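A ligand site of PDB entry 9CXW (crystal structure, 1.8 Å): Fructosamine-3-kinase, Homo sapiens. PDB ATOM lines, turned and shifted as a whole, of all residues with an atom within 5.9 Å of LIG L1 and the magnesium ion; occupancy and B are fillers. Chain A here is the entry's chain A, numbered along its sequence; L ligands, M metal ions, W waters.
The side-chain amino group of Lys 42 lies within salt-bridge range of an oxygen (O4) of LIG L1. The backbone NH (N) of Leu 92 is in hydrogen-bond range of a nitrogen (N4) of LIG L1, at 2.8 Å. The backbone carbonyl oxygen of Glu 90 is in hydrogen-bond range of a nitrogen (N3) of LIG L1 (2.9 Å). O3 of LIG L1 sits close to O of Ile 26 (2.9 Å). An oxygen (O9) of LIG L1 is in hydrogen-bond range of the side-chain hydroxyl of Tyr 215. O3 of LIG L1 sits close to N of Glu 28 (3.4 Å). The side-chain sulfur (SD) of Met 89 sits close to a nitrogen (N3) of LIG L1 (3.5 Å). O6 of LG2 L2 lies within hydrogen-bond range of OD2 of Asp 199, at 2.6 Å.
The side-chain carboxylate (OD1) of Asp 216 lies within salt-bridge range of the side-chain amino group (NZ) of Lys 42. N of Tyr 215 is in hydrogen-bond range of O of Asn 204 (3.0 Å). NE1 of Trp 201 sits close to ND2 of Asn 204 (3.4 Å). The side-chain amide nitrogen (ND2) of Asn 204 sits at hydrogen-bond distance from the backbone carbonyl oxygen (O) of Asp 199 (2.9 Å). The side-chain amino group of Lys 42 lies within salt-bridge range of the side-chain carboxylate of Glu 56 (2.8 Å). The side-chain hydroxyl of Tyr 215 lies within hydrogen-bond range of the backbone carbonyl oxygen of Gly 203 (2.8 Å). The backbone carbonyl oxygen (O) of Met 89 lies within hydrogen-bond range of the backbone NH (N) of Phe 40.
O of Cys 25 sits close to O3 of LIG L1 (3.3 Å). O of Ser 27 lies close to O3 of LIG L1 (3.5 Å). Merely in contact with LIG L1: Met 94, His 91, Pro 72 and Phe 40. Along chain A the residues within 4 Å of LIG L1 span positions 25 to 216. The nearest printed residue that does not touch LIG L1 is Gly 203 (4.01 Å).
Two residues have an atom within 4 Å of the magnesium ion: Asn 204 and Asp 216. The nearest printed residue that does not touch the magnesium ion is Trp 201 (4.4 Å).
O5 of LIG L1 binds the magnesium ion. Water W4 is bound to the magnesium ion, at 2.2 Å. OD2 of Asp 216 binds the magnesium ion (2.3 Å). The magnesium ion is bound by water W1 (2.3 Å). The magnesium ion is bound by the side-chain amide oxygen (OD1) of Asn 204. The magnesium ion is bound by O1 of LIG L1, 2.4 Å away. The magnesium ion has six donor atoms within binding distance.
Water W4 lies within hydrogen-bond range of O6 of LG2 L2 (2.5 Å), NE1 of Trp 201 (3.0 Å) and ND2 of Asn 204 (3.4 Å). Water W2 bridges O4 of LIG L1 (2.8 Å) and SD of Met 89 (3.3 Å). Water W3 lies within hydrogen-bond range of O10 of LIG L1 (2.8 Å) and SG of Cys 25 (3.5 Å).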
ATOM      1  N   CYS A  25     -17.346   2.772 -14.044  1.00  0.00           N
ATOM      2  CA  CYS A  25     -17.163   1.323 -14.007  1.00  0.00           C
ATOM      3  C   CYS A  25     -15.722   1.002 -13.602  1.00  0.00           C
ATOM      4  O   CYS A  25     -14.965   1.925 -13.307  1.00  0.00           O
ATOM      5  CB  CYS A  25     -17.488   0.710 -15.377  1.00  0.00           C
ATOM      6  SG  CYS A  25     -17.298  -1.071 -15.490  1.00  0.00           S
ATOM      7  N   ILE A  26     -15.354  -0.277 -13.562  1.00  0.00           N
ATOM      8  CA  ILE A  26     -14.009  -0.724 -13.218  1.00  0.00           C
ATOM      9  C   ILE A  26     -13.588  -0.197 -11.840  1.00  0.00           C
ATOM     10  O   ILE A  26     -12.385  -0.053 -11.575  1.00  0.00           O
ATOM     11  CB  ILE A  26     -12.995  -0.298 -14.308  1.00  0.00           C
ATOM     12  N   SER A  27     -14.566   0.083 -10.974  1.00  0.00           N
ATOM     13  CA  SER A  27     -14.350   0.722  -9.666  1.00  0.00           C
ATOM     14  C   SER A  27     -13.810   2.154  -9.823  1.00  0.00           C
ATOM     15  O   SER A  27     -12.752   2.513  -9.309  1.00  0.00           O
ATOM     16  CB  SER A  27     -13.434  -0.119  -8.762  1.00  0.00           C
ATOM     17  N   GLU A  28     -14.525   2.939 -10.634  1.00  0.00           N
ATOM     18  CA  GLU A  28     -14.214   4.348 -10.839  1.00  0.00           C
ATOM     19  C   GLU A  28     -15.326   5.273 -10.379  1.00  0.00           C
ATOM     20  O   GLU A  28     -15.391   5.670  -9.210  1.00  0.00           O
ATOM     21  CB  GLU A  28     -13.919   4.636 -12.320  1.00  0.00           C
ATOM     22  N   GLY A  29     -16.161   5.670 -11.352  1.00  0.00           N
ATOM     23  CA  GLY A  29     -17.251   6.608 -11.128  1.00  0.00           C
ATOM     24  C   GLY A  29     -18.468   6.281 -11.974  1.00  0.00           C
ATOM     25  O   GLY A  29     -18.740   5.121 -12.288  1.00  0.00           O
ATOM     26  N   ALA A  31     -21.471   8.083 -15.031  1.00  0.00           N
ATOM     27  CA  ALA A  31     -21.758   9.012 -16.098  1.00  0.00           C
ATOM     28  C   ALA A  31     -22.966   9.820 -15.694  1.00  0.00           C
ATOM     29  O   ALA A  31     -23.842   9.303 -14.992  1.00  0.00           O
ATOM     30  CB  ALA A  31     -22.025   8.266 -17.408  1.00  0.00           C
ATOM     31  N   PHE A  40     -18.417  12.313 -17.791  1.00  0.00           N
ATOM     32  CA  PHE A  40     -18.098  11.116 -17.058  1.00  0.00           C
ATOM     33  C   PHE A  40     -17.266  11.527 -15.857  1.00  0.00           C
ATOM     34  O   PHE A  40     -16.368  12.352 -15.979  1.00  0.00           O
ATOM     35  CB  PHE A  40     -17.366  10.090 -17.953  1.00  0.00           C
ATOM     36  CG  PHE A  40     -17.163   8.766 -17.275  1.00  0.00           C
ATOM     37  CD1 PHE A  40     -18.194   7.829 -17.232  1.00  0.00           C
ATOM     38  CD2 PHE A  40     -15.972   8.487 -16.637  1.00  0.00           C
ATOM     39  CE1 PHE A  40     -17.998   6.609 -16.574  1.00  0.00           C
ATOM     40  CE2 PHE A  40     -15.788   7.272 -15.985  1.00  0.00           C
ATOM     41  CZ  PHE A  40     -16.801   6.340 -15.955  1.00  0.00           C
ATOM     42  N   LYS A  42     -15.031  10.328 -12.502  1.00  0.00           N
ATOM     43  CA  LYS A  42     -14.295   9.317 -11.746  1.00  0.00           C
ATOM     44  C   LYS A  42     -14.130   9.806 -10.322  1.00  0.00           C
ATOM     45  O   LYS A  42     -13.727  10.944 -10.103  1.00  0.00           O
ATOM     46  CB  LYS A  42     -12.894   9.101 -12.329  1.00  0.00           C
ATOM     47  CG  LYS A  42     -12.827   8.240 -13.510  1.00  0.00           C
ATOM     48  CD  LYS A  42     -11.365   7.894 -13.626  1.00  0.00           C
ATOM     49  CE  LYS A  42     -11.007   7.473 -14.982  1.00  0.00           C
ATOM     50  NZ  LYS A  42      -9.633   6.905 -14.968  1.00  0.00           N
ATOM     51  N   GLU A  56      -3.134  11.884 -14.391  1.00  0.00           N
ATOM     52  CA  GLU A  56      -3.960  11.418 -15.494  1.00  0.00           C
ATOM     53  C   GLU A  56      -4.284  12.567 -16.410  1.00  0.00           C
ATOM     54  O   GLU A  56      -4.239  12.417 -17.642  1.00  0.00           O
ATOM     55  CB  GLU A  56      -5.257  10.756 -14.992  1.00  0.00           C
ATOM     56  CG  GLU A  56      -6.102  10.054 -16.099  1.00  0.00           C
ATOM     57  CD  GLU A  56      -7.329   9.298 -15.527  1.00  0.00           C
ATOM     58  OE1 GLU A  56      -7.439   9.183 -14.279  1.00  0.00           O
ATOM     59  OE2 GLU A  56      -8.179   8.824 -16.319  1.00  0.00           O
ATOM     60  N   PRO A  72     -10.477  10.940 -23.988  1.00  0.00           N
ATOM     61  CA  PRO A  72     -11.469  11.854 -23.388  1.00  0.00           C
ATOM     62  C   PRO A  72     -10.800  13.168 -22.969  1.00  0.00           C
ATOM     63  O   PRO A  72      -9.661  13.184 -22.477  1.00  0.00           O
ATOM     64  CB  PRO A  72     -12.026  11.061 -22.183  1.00  0.00           C
ATOM     65  CG  PRO A  72     -11.062   9.965 -21.907  1.00  0.00           C
ATOM     66  CD  PRO A  72     -10.338   9.675 -23.235  1.00  0.00           C
ATOM     67  N   MET A  89     -14.614  14.473 -16.957  1.00  0.00           N
ATOM     68  CA  MET A  89     -14.107  14.503 -18.313  1.00  0.00           C
ATOM     69  C   MET A  89     -15.276  14.389 -19.284  1.00  0.00           C
ATOM     70  O   MET A  89     -16.403  14.083 -18.903  1.00  0.00           O
ATOM     71  CB  MET A  89     -13.056  13.388 -18.500  1.00  0.00           C
ATOM     72  CG  MET A  89     -13.599  11.987 -18.670  1.00  0.00           C
ATOM     73  SD  MET A  89     -12.276  10.748 -18.490  1.00  0.00           S
ATOM     74  CE  MET A  89     -12.240  10.532 -16.721  1.00  0.00           C
ATOM     75  N   GLU A  90     -14.997  14.697 -20.547  1.00  0.00           N
ATOM     76  CA  GLU A  90     -15.974  14.557 -21.620  1.00  0.00           C
ATOM     77  C   GLU A  90     -16.459  13.114 -21.687  1.00  0.00           C
ATOM     78  O   GLU A  90     -15.666  12.171 -21.584  1.00  0.00           O
ATOM     79  CB  GLU A  90     -15.319  14.974 -22.941  1.00  0.00           C
ATOM     80  CG  GLU A  90     -15.851  14.288 -24.193  1.00  0.00           C
ATOM     81  CD  GLU A  90     -14.886  14.380 -25.373  1.00  0.00           C
ATOM     82  OE1 GLU A  90     -13.671  14.160 -25.158  1.00  0.00           O
ATOM     83  OE2 GLU A  90     -15.338  14.654 -26.508  1.00  0.00           O
ATOM     84  N   HIS A  91     -17.761  12.931 -21.818  1.00  0.00           N
ATOM     85  CA  HIS A  91     -18.297  11.596 -21.962  1.00  0.00           C
ATOM     86  C   HIS A  91     -18.190  11.131 -23.409  1.00  0.00           C
ATOM     87  O   HIS A  91     -18.471  11.891 -24.339  1.00  0.00           O
ATOM     88  CB  HIS A  91     -19.762  11.551 -21.516  1.00  0.00           C
ATOM     89  CG  HIS A  91     -20.405  10.204 -21.675  1.00  0.00           C
ATOM     90  ND1 HIS A  91     -20.994   9.818 -22.853  1.00  0.00           N
ATOM     91  CD2 HIS A  91     -20.554   9.176 -20.824  1.00  0.00           C
ATOM     92  CE1 HIS A  91     -21.462   8.589 -22.727  1.00  0.00           C
ATOM     93  NE2 HIS A  91     -21.230   8.184 -21.491  1.00  0.00           N
ATOM     94  N   LEU A  92     -17.777   9.877 -23.591  1.00  0.00           N
ATOM     95  CA  LEU A  92     -17.654   9.256 -24.907  1.00  0.00           C
ATOM     96  C   LEU A  92     -18.514   7.994 -24.899  1.00  0.00           C
ATOM     97  O   LEU A  92     -18.416   7.184 -23.961  1.00  0.00           O
ATOM     98  CB  LEU A  92     -16.192   8.895 -25.223  1.00  0.00           C
ATOM     99  CG  LEU A  92     -15.253  10.084 -25.367  1.00  0.00           C
ATOM    100  CD1 LEU A  92     -13.799   9.640 -25.718  1.00  0.00           C
ATOM    101  CD2 LEU A  92     -15.782  11.077 -26.367  1.00  0.00           C
ATOM    102  N   LYS A  93     -19.364   7.842 -25.918  1.00  0.00           N
ATOM    103  CA  LYS A  93     -20.102   6.589 -26.079  1.00  0.00           C
ATOM    104  C   LYS A  93     -19.124   5.565 -26.622  1.00  0.00           C
ATOM    105  O   LYS A  93     -18.519   5.779 -27.668  1.00  0.00           O
ATOM    106  CB  LYS A  93     -21.283   6.783 -27.044  1.00  0.00           C
ATOM    107  N   MET A  94     -18.966   4.445 -25.907  1.00  0.00           N
ATOM    108  CA  MET A  94     -17.786   3.603 -26.098  1.00  0.00           C
ATOM    109  C   MET A  94     -18.243   2.155 -26.140  1.00  0.00           C
ATOM    110  O   MET A  94     -19.038   1.736 -25.282  1.00  0.00           O
ATOM    111  CB  MET A  94     -16.855   3.820 -24.883  1.00  0.00           C
ATOM    112  CG  MET A  94     -15.806   4.936 -25.005  1.00  0.00           C
ATOM    113  SD  MET A  94     -14.732   4.886 -23.569  1.00  0.00           S
ATOM    114  CE  MET A  94     -15.037   3.201 -23.076  1.00  0.00           C
ATOM    115  N   ASP A 199      -0.462   2.286 -20.001  1.00  0.00           N
ATOM    116  CA  ASP A 199      -1.283   1.283 -19.350  1.00  0.00           C
ATOM    117  C   ASP A 199      -2.279   0.705 -20.355  1.00  0.00           C
ATOM    118  O   ASP A 199      -3.492   0.638 -20.095  1.00  0.00           O
ATOM    119  CB  ASP A 199      -2.024   1.889 -18.152  1.00  0.00           C
ATOM    120  CG  ASP A 199      -2.561   0.813 -17.167  1.00  0.00           C
ATOM    121  OD1 ASP A 199      -2.037  -0.324 -17.191  1.00  0.00           O
ATOM    122  OD2 ASP A 199      -3.481   1.126 -16.393  1.00  0.00           O
ATOM    123  N   TRP A 201      -3.825  -1.813 -21.429  1.00  0.00           N
ATOM    124  CA  TRP A 201      -4.493  -3.115 -21.519  1.00  0.00           C
ATOM    125  C   TRP A 201      -5.892  -2.995 -22.172  1.00  0.00           C
ATOM    126  O   TRP A 201      -6.411  -1.900 -22.448  1.00  0.00           O
ATOM    127  CB  TRP A 201      -4.552  -3.801 -20.145  1.00  0.00           C
ATOM    128  CG  TRP A 201      -5.619  -3.316 -19.253  1.00  0.00           C
ATOM    129  CD1 TRP A 201      -5.703  -2.071 -18.676  1.00  0.00           C
ATOM    130  CD2 TRP A 201      -6.779  -4.048 -18.781  1.00  0.00           C
ATOM    131  NE1 TRP A 201      -6.852  -1.993 -17.883  1.00  0.00           N
ATOM    132  CE2 TRP A 201      -7.527  -3.166 -17.955  1.00  0.00           C
ATOM    133  CE3 TRP A 201      -7.273  -5.347 -18.999  1.00  0.00           C
ATOM    134  CZ2 TRP A 201      -8.749  -3.563 -17.304  1.00  0.00           C
ATOM    135  CZ3 TRP A 201      -8.479  -5.726 -18.366  1.00  0.00           C
ATOM    136  CH2 TRP A 201      -9.183  -4.831 -17.531  1.00  0.00           C
ATOM    137  N   GLY A 203      -8.819  -3.338 -21.322  1.00  0.00           N
ATOM    138  CA  GLY A 203      -9.852  -2.611 -20.606  1.00  0.00           C
ATOM    139  C   GLY A 203      -9.705  -1.113 -20.643  1.00  0.00           C
ATOM    140  O   GLY A 203     -10.614  -0.417 -20.169  1.00  0.00           O
ATOM    141  N   ASN A 204      -8.587  -0.588 -21.167  1.00  0.00           N
ATOM    142  CA  ASN A 204      -8.363   0.855 -21.269  1.00  0.00           C
ATOM    143  C   ASN A 204      -8.451   1.352 -22.703  1.00  0.00           C
ATOM    144  O   ASN A 204      -7.988   2.466 -23.015  1.00  0.00           O
ATOM    145  CB  ASN A 204      -7.015   1.222 -20.672  1.00  0.00           C
ATOM    146  CG  ASN A 204      -7.035   1.231 -19.148  1.00  0.00           C
ATOM    147  OD1 ASN A 204      -8.106   1.239 -18.537  1.00  0.00           O
ATOM    148  ND2 ASN A 204      -5.875   1.191 -18.540  1.00  0.00           N
ATOM    149  N   TYR A 215      -7.916   5.501 -22.983  1.00  0.00           N
ATOM    150  CA  TYR A 215      -8.164   6.308 -21.786  1.00  0.00           C
ATOM    151  C   TYR A 215      -7.453   5.697 -20.584  1.00  0.00           C
ATOM    152  O   TYR A 215      -6.776   4.668 -20.692  1.00  0.00           O
ATOM    153  CB  TYR A 215      -9.678   6.416 -21.522  1.00  0.00           C
ATOM    154  CG  TYR A 215     -10.350   5.071 -21.553  1.00  0.00           C
ATOM    155  CD1 TYR A 215     -10.858   4.556 -22.745  1.00  0.00           C
ATOM    156  CD2 TYR A 215     -10.486   4.299 -20.399  1.00  0.00           C
ATOM    157  CE1 TYR A 215     -11.509   3.295 -22.768  1.00  0.00           C
ATOM    158  CE2 TYR A 215     -11.127   3.060 -20.423  1.00  0.00           C
ATOM    159  CZ  TYR A 215     -11.625   2.577 -21.613  1.00  0.00           C
ATOM    160  OH  TYR A 215     -12.218   1.353 -21.653  1.00  0.00           O
ATOM    161  N   ASP A 216      -7.587   6.363 -19.429  1.00  0.00           N
ATOM    162  CA  ASP A 216      -6.923   5.939 -18.200  1.00  0.00           C
ATOM    163  C   ASP A 216      -5.422   5.782 -18.394  1.00  0.00           C
ATOM    164  O   ASP A 216      -4.842   4.752 -18.001  1.00  0.00           O
ATOM    165  CB  ASP A 216      -7.535   4.623 -17.717  1.00  0.00           C
ATOM    166  CG  ASP A 216      -7.255   4.324 -16.206  1.00  0.00           C
ATOM    167  OD1 ASP A 216      -6.901   5.252 -15.431  1.00  0.00           O
ATOM    168  OD2 ASP A 216      -7.464   3.145 -15.797  1.00  0.00           O
HETATM  169  P1  LIG L   1     -10.795   2.848 -13.753  1.00  0.00           P
HETATM  170  O1  LIG L   1     -10.294   1.596 -14.434  1.00  0.00           O
HETATM  171  O2  LIG L   1      -9.711   3.796 -13.268  1.00  0.00           O
HETATM  172  O3  LIG L   1     -11.804   2.543 -12.675  1.00  0.00           O
HETATM  173  P2  LIG L   1     -11.341   3.809 -16.495  1.00  0.00           P
HETATM  174  O4  LIG L   1     -10.941   5.225 -16.838  1.00  0.00           O
HETATM  175  O5  LIG L   1     -10.483   2.670 -16.990  1.00  0.00           O
HETATM  176  O6  LIG L   1     -11.626   3.701 -14.886  1.00  0.00           O
HETATM  177  O7  LIG L   1     -12.821   3.599 -17.118  1.00  0.00           O
HETATM  178  C1  LIG L   1     -13.502   2.345 -16.938  1.00  0.00           C
HETATM  179  C2  LIG L   1     -14.788   2.312 -17.759  1.00  0.00           C
HETATM  180  O8  LIG L   1     -15.495   3.525 -17.558  1.00  0.00           O
HETATM  181  C3  LIG L   1     -14.556   2.253 -19.261  1.00  0.00           C
HETATM  182  O9  LIG L   1     -14.375   0.923 -19.748  1.00  0.00           O
HETATM  183  C4  LIG L   1     -15.761   2.969 -19.853  1.00  0.00           C
HETATM  184  O10 LIG L   1     -16.910   2.140 -20.143  1.00  0.00           O
HETATM  185  C5  LIG L   1     -16.113   3.965 -18.766  1.00  0.00           C
HETATM  186  N1  LIG L   1     -15.541   5.288 -19.126  1.00  0.00           N
HETATM  187  C6  LIG L   1     -14.325   5.740 -18.755  1.00  0.00           C
HETATM  188  N2  LIG L   1     -14.106   6.997 -19.203  1.00  0.00           N
HETATM  189  C7  LIG L   1     -15.182   7.347 -19.913  1.00  0.00           C
HETATM  190  C8  LIG L   1     -15.590   8.546 -20.670  1.00  0.00           C
HETATM  191  N3  LIG L   1     -14.747   9.599 -20.714  1.00  0.00           N
HETATM  192  N4  LIG L   1     -16.818   8.554 -21.267  1.00  0.00           N
HETATM  193  C9  LIG L   1     -17.614   7.484 -21.163  1.00  0.00           C
HETATM  194  N5  LIG L   1     -17.283   6.357 -20.498  1.00  0.00           N
HETATM  195  C10 LIG L   1     -16.131   6.234 -19.841  1.00  0.00           C
HETATM  196  N1  LG2 L   2      -5.495  -5.498 -14.523  1.00  0.00           N
HETATM  197  C1  LG2 L   2      -5.060  -4.203 -15.173  1.00  0.00           C
HETATM  198  C2  LG2 L   2      -5.255  -2.834 -14.421  1.00  0.00           C
HETATM  199  O1  LG2 L   2      -6.087  -2.642 -13.514  1.00  0.00           O
HETATM  200  C3  LG2 L   2      -6.853  -5.494 -13.981  1.00  0.00           C
HETATM  201  C4  LG2 L   2      -7.252  -6.861 -13.395  1.00  0.00           C
HETATM  202  C5  LG2 L   2      -6.211  -7.821 -15.333  1.00  0.00           C
HETATM  203  C6  LG2 L   2      -5.429  -6.522 -15.597  1.00  0.00           C
HETATM  204  C7  LG2 L   2      -4.384  -1.641 -14.949  1.00  0.00           C
HETATM  205  C8  LG2 L   2      -2.974  -1.462 -14.278  1.00  0.00           C
HETATM  206  C9  LG2 L   2      -2.802  -1.992 -12.802  1.00  0.00           C
HETATM  207  C10 LG2 L   2      -3.522  -1.136 -11.748  1.00  0.00           C
HETATM  208  O2  LG2 L   2      -6.469  -7.952 -13.937  1.00  0.00           O
HETATM  209  O3  LG2 L   2      -4.948  -1.237 -11.833  1.00  0.00           O
HETATM  210  O4  LG2 L   2      -3.217  -3.356 -12.674  1.00  0.00           O
HETATM  211  O5  LG2 L   2      -1.983  -2.050 -15.151  1.00  0.00           O
HETATM  212  O6  LG2 L   2      -5.093  -0.361 -14.911  1.00  0.00           O
HETATM  213 MG    MG M   1      -8.968   1.514 -16.383  1.00  0.00          MG
HETATM  214  O   HOH W   1     -10.479  -0.017 -17.230  1.00  0.00           O
HETATM  215  O   HOH W   2     -11.346   7.544 -18.328  1.00  0.00           O
HETATM  216  O   HOH W   3     -18.444   0.411 -18.492  1.00  0.00           O
HETATM  217  O   HOH W   4      -7.407   0.093 -15.767  1.00  0.00           O
